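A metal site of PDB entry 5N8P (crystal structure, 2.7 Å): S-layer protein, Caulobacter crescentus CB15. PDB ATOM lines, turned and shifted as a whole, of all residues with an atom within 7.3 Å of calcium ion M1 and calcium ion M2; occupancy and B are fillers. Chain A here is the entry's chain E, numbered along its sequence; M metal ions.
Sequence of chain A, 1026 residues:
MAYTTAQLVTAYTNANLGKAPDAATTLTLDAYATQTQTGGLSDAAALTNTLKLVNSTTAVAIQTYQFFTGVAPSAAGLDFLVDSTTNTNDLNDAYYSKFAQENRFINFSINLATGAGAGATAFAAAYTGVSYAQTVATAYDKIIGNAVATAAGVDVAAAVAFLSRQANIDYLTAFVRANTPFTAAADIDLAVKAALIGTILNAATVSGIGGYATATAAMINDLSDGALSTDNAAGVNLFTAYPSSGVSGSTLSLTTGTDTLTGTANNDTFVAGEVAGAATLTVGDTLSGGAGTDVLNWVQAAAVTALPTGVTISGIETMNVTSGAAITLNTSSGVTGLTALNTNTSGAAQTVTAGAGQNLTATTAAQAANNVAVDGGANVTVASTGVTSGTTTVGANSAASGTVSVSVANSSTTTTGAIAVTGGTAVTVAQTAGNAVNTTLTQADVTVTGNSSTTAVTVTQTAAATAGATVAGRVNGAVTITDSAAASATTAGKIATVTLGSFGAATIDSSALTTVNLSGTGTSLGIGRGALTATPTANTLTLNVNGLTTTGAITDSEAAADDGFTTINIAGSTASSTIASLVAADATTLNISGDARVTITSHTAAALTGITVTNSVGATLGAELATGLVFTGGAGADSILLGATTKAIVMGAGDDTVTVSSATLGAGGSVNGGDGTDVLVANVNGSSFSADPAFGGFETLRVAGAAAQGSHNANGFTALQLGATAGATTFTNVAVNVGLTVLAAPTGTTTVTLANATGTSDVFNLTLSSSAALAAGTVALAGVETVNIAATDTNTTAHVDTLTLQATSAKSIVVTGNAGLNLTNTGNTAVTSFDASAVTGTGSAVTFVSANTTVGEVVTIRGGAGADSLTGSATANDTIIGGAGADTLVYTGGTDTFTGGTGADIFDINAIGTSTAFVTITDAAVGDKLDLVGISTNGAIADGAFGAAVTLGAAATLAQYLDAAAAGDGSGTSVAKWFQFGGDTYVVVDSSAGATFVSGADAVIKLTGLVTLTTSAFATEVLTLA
Merely in contact with calcium ion M1: Ala 265 and Asp 268.
Within 4 Å of calcium ion M1: Ala 265, Asn 266, Asp 268, Gly 289, Gly 290, Ala 291 and Asp 294.
The nearest printed residue that does not touch calcium ion M1 is Thr 264 (4.1 Å).
Calcium ion M2 is bound by the side-chain carboxylate of Glu 317 (2.3 Å), the backbone carbonyl oxygen of Gly 315 (2.3 Å), the side-chain carboxylate of Asp 294 (2.6 Å), the backbone carbonyl oxygen of Ala 291 (2.7 Å) and the backbone carbonyl oxygen of Gly 290 (2.7 Å).
Calcium ion M2 has five donor atoms within binding distance.
Slightly farther from calcium ion M2 lies OE1 of Glu 317 (3.0 Å).
Residues that only touch calcium ion M2: Gly 292 (3.9 Å).
Of the 23 residues printed, 6 come within 4 Å of calcium ion M2.
Calcium ion M1 is bound by O of Gly 289, 2.4 Å away.
OD2 of Asp 294 is bound to calcium ion M1 (2.7 Å).
The side-chain carboxylate (OD1) of Asp 294 binds calcium ion M1 (2.7 Å).
O of Asn 266 is bound to calcium ion M1 (2.8 Å).
The backbone nitrogen (N) of Asn 266 is bound to calcium ion M1, at 2.9 Å.
Slightly farther from calcium ion M1 lies O of Ala 291 (3.1 Å).
N of Thr 293 lies within hydrogen-bond range of OE1 of Glu 317, at 3.4 Å.
The side-chain amide oxygen (OD1) of Asn 267 lies within hydrogen-bond range of the side-chain amide nitrogen (ND2) of Asn 266, at 3.0 Å.
N of Asp 268 lies close to OD2 of Asp 294, at 3.4 Å.
The backbone NH (N) of Asp 268 is in hydrogen-bond range of the backbone carbonyl oxygen (O) of Thr 293 (3.4 Å).
The backbone carbonyl oxygen (O) of Asp 268 lies within hydrogen-bond range of the backbone NH (N) of Val 295, at 3.2 Å.
N of Gly 289 sits at hydrogen-bond distance from O of Ser 314 (3.0 Å).
OG1 of Thr 264 is in hydrogen-bond range of OD2 of Asp 268 (2.5 Å).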
ATOM      1  N   GLY A 249      14.067  35.509 -20.861  1.00  0.00           N
ATOM      2  CA  GLY A 249      14.105  33.994 -20.808  1.00  0.00           C
ATOM      3  C   GLY A 249      13.422  33.298 -21.981  1.00  0.00           C
ATOM      4  O   GLY A 249      13.095  33.975 -22.975  1.00  0.00           O
ATOM      5  N   THR A 262      12.842  21.717 -19.136  1.00  0.00           N
ATOM      6  CA  THR A 262      13.936  22.280 -18.360  1.00  0.00           C
ATOM      7  C   THR A 262      14.236  23.716 -18.811  1.00  0.00           C
ATOM      8  O   THR A 262      14.559  23.951 -19.980  1.00  0.00           O
ATOM      9  CB  THR A 262      15.167  21.325 -18.373  1.00  0.00           C
ATOM     10  OG1 THR A 262      14.794  20.088 -17.767  1.00  0.00           O
ATOM     11  CG2 THR A 262      16.359  21.889 -17.577  1.00  0.00           C
ATOM     12  N   GLY A 263      14.146  24.657 -17.870  1.00  0.00           N
ATOM     13  CA  GLY A 263      14.264  26.106 -18.136  1.00  0.00           C
ATOM     14  C   GLY A 263      15.668  26.566 -18.490  1.00  0.00           C
ATOM     15  O   GLY A 263      16.599  25.765 -18.486  1.00  0.00           O
ATOM     16  N   THR A 264      15.829  27.852 -18.788  1.00  0.00           N
ATOM     17  CA  THR A 264      17.138  28.372 -19.210  1.00  0.00           C
ATOM     18  C   THR A 264      18.039  28.830 -18.078  1.00  0.00           C
ATOM     19  O   THR A 264      19.205  29.158 -18.326  1.00  0.00           O
ATOM     20  CB  THR A 264      17.060  29.535 -20.239  1.00  0.00           C
ATOM     21  OG1 THR A 264      16.131  30.534 -19.787  1.00  0.00           O
ATOM     22  CG2 THR A 264      16.703  29.040 -21.636  1.00  0.00           C
ATOM     23  N   ALA A 265      17.540  28.815 -16.840  1.00  0.00           N
ATOM     24  CA  ALA A 265      18.182  29.516 -15.721  1.00  0.00           C
ATOM     25  C   ALA A 265      18.095  31.036 -15.963  1.00  0.00           C
ATOM     26  O   ALA A 265      19.061  31.781 -15.872  1.00  0.00           O
ATOM     27  CB  ALA A 265      19.615  29.032 -15.442  1.00  0.00           C
ATOM     28  N   ASN A 266      16.871  31.474 -16.238  1.00  0.00           N
ATOM     29  CA  ASN A 266      16.557  32.831 -16.694  1.00  0.00           C
ATOM     30  C   ASN A 266      15.032  33.056 -16.521  1.00  0.00           C
ATOM     31  O   ASN A 266      14.333  32.199 -15.972  1.00  0.00           O
ATOM     32  CB  ASN A 266      16.964  32.984 -18.160  1.00  0.00           C
ATOM     33  CG  ASN A 266      17.827  34.180 -18.423  1.00  0.00           C
ATOM     34  OD1 ASN A 266      19.013  34.051 -18.703  1.00  0.00           O
ATOM     35  ND2 ASN A 266      17.234  35.368 -18.381  1.00  0.00           N
ATOM     36  N   ASN A 267      14.541  34.198 -17.025  1.00  0.00           N
ATOM     37  CA  ASN A 267      13.132  34.659 -16.954  1.00  0.00           C
ATOM     38  C   ASN A 267      12.095  33.757 -17.653  1.00  0.00           C
ATOM     39  O   ASN A 267      11.170  34.258 -18.322  1.00  0.00           O
ATOM     40  CB  ASN A 267      12.984  36.105 -17.520  1.00  0.00           C
ATOM     41  CG  ASN A 267      14.246  36.970 -17.382  1.00  0.00           C
ATOM     42  OD1 ASN A 267      14.923  37.269 -18.384  1.00  0.00           O
ATOM     43  ND2 ASN A 267      14.564  37.396 -16.143  1.00  0.00           N
ATOM     44  N   ASP A 268      12.204  32.439 -17.500  1.00  0.00           N
ATOM     45  CA  ASP A 268      11.363  31.574 -18.320  1.00  0.00           C
ATOM     46  C   ASP A 268       9.992  31.195 -17.751  1.00  0.00           C
ATOM     47  O   ASP A 268       9.778  31.185 -16.526  1.00  0.00           O
ATOM     48  CB  ASP A 268      12.133  30.413 -19.023  1.00  0.00           C
ATOM     49  CG  ASP A 268      13.092  29.701 -18.122  1.00  0.00           C
ATOM     50  OD1 ASP A 268      12.633  28.911 -17.292  1.00  0.00           O
ATOM     51  OD2 ASP A 268      14.307  29.906 -18.255  1.00  0.00           O
ATOM     52  N   THR A 269       9.045  30.977 -18.660  1.00  0.00           N
ATOM     53  CA  THR A 269       7.629  30.808 -18.332  1.00  0.00           C
ATOM     54  C   THR A 269       7.128  29.488 -18.960  1.00  0.00           C
ATOM     55  O   THR A 269       7.469  29.145 -20.097  1.00  0.00           O
ATOM     56  CB  THR A 269       6.782  32.040 -18.781  1.00  0.00           C
ATOM     57  OG1 THR A 269       6.474  31.925 -20.151  1.00  0.00           O
ATOM     58  CG2 THR A 269       7.512  33.430 -18.569  1.00  0.00           C
ATOM     59  N   PHE A 270       6.316  28.757 -18.202  1.00  0.00           N
ATOM     60  CA  PHE A 270       5.879  27.394 -18.549  1.00  0.00           C
ATOM     61  C   PHE A 270       4.379  27.404 -18.758  1.00  0.00           C
ATOM     62  O   PHE A 270       3.659  27.735 -17.833  1.00  0.00           O
ATOM     63  CB  PHE A 270       6.145  26.437 -17.403  1.00  0.00           C
ATOM     64  CG  PHE A 270       7.552  25.966 -17.284  1.00  0.00           C
ATOM     65  CD1 PHE A 270       7.860  24.647 -17.560  1.00  0.00           C
ATOM     66  CD2 PHE A 270       8.562  26.800 -16.799  1.00  0.00           C
ATOM     67  CE1 PHE A 270       9.169  24.185 -17.427  1.00  0.00           C
ATOM     68  CE2 PHE A 270       9.871  26.344 -16.653  1.00  0.00           C
ATOM     69  CZ  PHE A 270      10.171  25.028 -16.979  1.00  0.00           C
ATOM     70  N   SER A 288      11.254  21.741 -14.578  1.00  0.00           N
ATOM     71  CA  SER A 288      12.494  22.174 -13.935  1.00  0.00           C
ATOM     72  C   SER A 288      12.865  23.602 -14.361  1.00  0.00           C
ATOM     73  O   SER A 288      12.943  23.880 -15.557  1.00  0.00           O
ATOM     74  CB  SER A 288      13.601  21.189 -14.297  1.00  0.00           C
ATOM     75  OG  SER A 288      14.675  21.261 -13.394  1.00  0.00           O
ATOM     76  N   GLY A 289      13.108  24.492 -13.384  1.00  0.00           N
ATOM     77  CA  GLY A 289      13.276  25.922 -13.646  1.00  0.00           C
ATOM     78  C   GLY A 289      14.632  26.556 -13.974  1.00  0.00           C
ATOM     79  O   GLY A 289      14.741  27.266 -14.987  1.00  0.00           O
ATOM     80  N   GLY A 290      15.651  26.380 -13.102  1.00  0.00           N
ATOM     81  CA  GLY A 290      16.933  27.137 -13.178  1.00  0.00           C
ATOM     82  C   GLY A 290      16.880  28.430 -12.364  1.00  0.00           C
ATOM     83  O   GLY A 290      16.439  28.398 -11.219  1.00  0.00           O
ATOM     84  N   ALA A 291      17.294  29.567 -12.931  1.00  0.00           N
ATOM     85  CA  ALA A 291      17.260  30.883 -12.232  1.00  0.00           C
ATOM     86  C   ALA A 291      15.870  31.486 -11.884  1.00  0.00           C
ATOM     87  O   ALA A 291      14.854  31.071 -12.405  1.00  0.00           O
ATOM     88  CB  ALA A 291      18.145  31.907 -12.940  1.00  0.00           C
ATOM     89  N   GLY A 292      15.851  32.496 -11.016  1.00  0.00           N
ATOM     90  CA  GLY A 292      14.636  32.963 -10.299  1.00  0.00           C
ATOM     91  C   GLY A 292      13.654  33.967 -10.915  1.00  0.00           C
ATOM     92  O   GLY A 292      13.221  34.944 -10.267  1.00  0.00           O
ATOM     93  N   THR A 293      13.301  33.723 -12.172  1.00  0.00           N
ATOM     94  CA  THR A 293      12.206  34.455 -12.771  1.00  0.00           C
ATOM     95  C   THR A 293      11.263  33.433 -13.418  1.00  0.00           C
ATOM     96  O   THR A 293      10.849  33.600 -14.582  1.00  0.00           O
ATOM     97  CB  THR A 293      12.667  35.651 -13.694  1.00  0.00           C
ATOM     98  OG1 THR A 293      13.958  35.414 -14.272  1.00  0.00           O
ATOM     99  CG2 THR A 293      12.715  37.003 -12.930  1.00  0.00           C
ATOM    100  N   ASP A 294      10.932  32.377 -12.657  1.00  0.00           N
ATOM    101  CA  ASP A 294      10.171  31.239 -13.218  1.00  0.00           C
ATOM    102  C   ASP A 294       8.683  31.136 -12.856  1.00  0.00           C
ATOM    103  O   ASP A 294       8.298  31.134 -11.684  1.00  0.00           O
ATOM    104  CB  ASP A 294      10.888  29.899 -12.991  1.00  0.00           C
ATOM    105  CG  ASP A 294      12.220  29.773 -13.760  1.00  0.00           C
ATOM    106  OD1 ASP A 294      13.118  29.077 -13.254  1.00  0.00           O
ATOM    107  OD2 ASP A 294      12.402  30.373 -14.841  1.00  0.00           O
ATOM    108  N   VAL A 295       7.873  31.020 -13.907  1.00  0.00           N
ATOM    109  CA  VAL A 295       6.413  31.056 -13.832  1.00  0.00           C
ATOM    110  C   VAL A 295       5.822  29.801 -14.475  1.00  0.00           C
ATOM    111  O   VAL A 295       6.253  29.410 -15.551  1.00  0.00           O
ATOM    112  CB  VAL A 295       5.834  32.282 -14.600  1.00  0.00           C
ATOM    113  CG1 VAL A 295       4.398  32.537 -14.175  1.00  0.00           C
ATOM    114  CG2 VAL A 295       6.697  33.559 -14.418  1.00  0.00           C
ATOM    115  N   SER A 314       9.689  21.706  -9.924  1.00  0.00           N
ATOM    116  CA  SER A 314      10.888  22.044  -9.201  1.00  0.00           C
ATOM    117  C   SER A 314      11.566  23.266  -9.807  1.00  0.00           C
ATOM    118  O   SER A 314      11.688  23.381 -11.036  1.00  0.00           O
ATOM    119  CB  SER A 314      11.801  20.823  -9.178  1.00  0.00           C
ATOM    120  OG  SER A 314      13.134  21.170  -9.492  1.00  0.00           O
ATOM    121  N   GLY A 315      12.012  24.177  -8.936  1.00  0.00           N
ATOM    122  CA  GLY A 315      12.774  25.347  -9.374  1.00  0.00           C
ATOM    123  C   GLY A 315      11.906  26.416 -10.011  1.00  0.00           C
ATOM    124  O   GLY A 315      12.430  27.337 -10.651  1.00  0.00           O
ATOM    125  N   ILE A 316      10.581  26.306  -9.804  1.00  0.00           N
ATOM    126  CA  ILE A 316       9.652  27.287 -10.334  1.00  0.00           C
ATOM    127  C   ILE A 316       8.984  28.033  -9.192  1.00  0.00           C
ATOM    128  O   ILE A 316       8.346  27.428  -8.324  1.00  0.00           O
ATOM    129  CB  ILE A 316       8.618  26.664 -11.298  1.00  0.00           C
ATOM    130  CG1 ILE A 316       9.324  25.813 -12.359  1.00  0.00           C
ATOM    131  CG2 ILE A 316       7.762  27.734 -11.926  1.00  0.00           C
ATOM    132  CD1 ILE A 316       8.407  24.988 -13.236  1.00  0.00           C
ATOM    133  N   GLU A 317       9.113  29.357  -9.240  1.00  0.00           N
ATOM    134  CA  GLU A 317       8.797  30.250  -8.111  1.00  0.00           C
ATOM    135  C   GLU A 317       7.319  30.626  -7.983  1.00  0.00           C
ATOM    136  O   GLU A 317       6.793  30.698  -6.865  1.00  0.00           O
ATOM    137  CB  GLU A 317       9.653  31.536  -8.190  1.00  0.00           C
ATOM    138  CG  GLU A 317      11.156  31.339  -7.978  1.00  0.00           C
ATOM    139  CD  GLU A 317      11.898  30.749  -9.190  1.00  0.00           C
ATOM    140  OE1 GLU A 317      11.795  31.251 -10.337  1.00  0.00           O
ATOM    141  OE2 GLU A 317      12.631  29.747  -8.971  1.00  0.00           O
ATOM    142  N   GLY A 337      10.593  24.663  -4.124  1.00  0.00           N
ATOM    143  CA  GLY A 337      11.157  25.919  -4.609  1.00  0.00           C
ATOM    144  C   GLY A 337      10.099  26.972  -4.951  1.00  0.00           C
ATOM    145  O   GLY A 337      10.430  28.063  -5.458  1.00  0.00           O
HETATM  146 CA    CA M   1      14.981  29.640 -15.141  1.00  0.00          CA
HETATM  147 CA    CA M   2      13.852  29.172 -10.789  1.00  0.00          CA
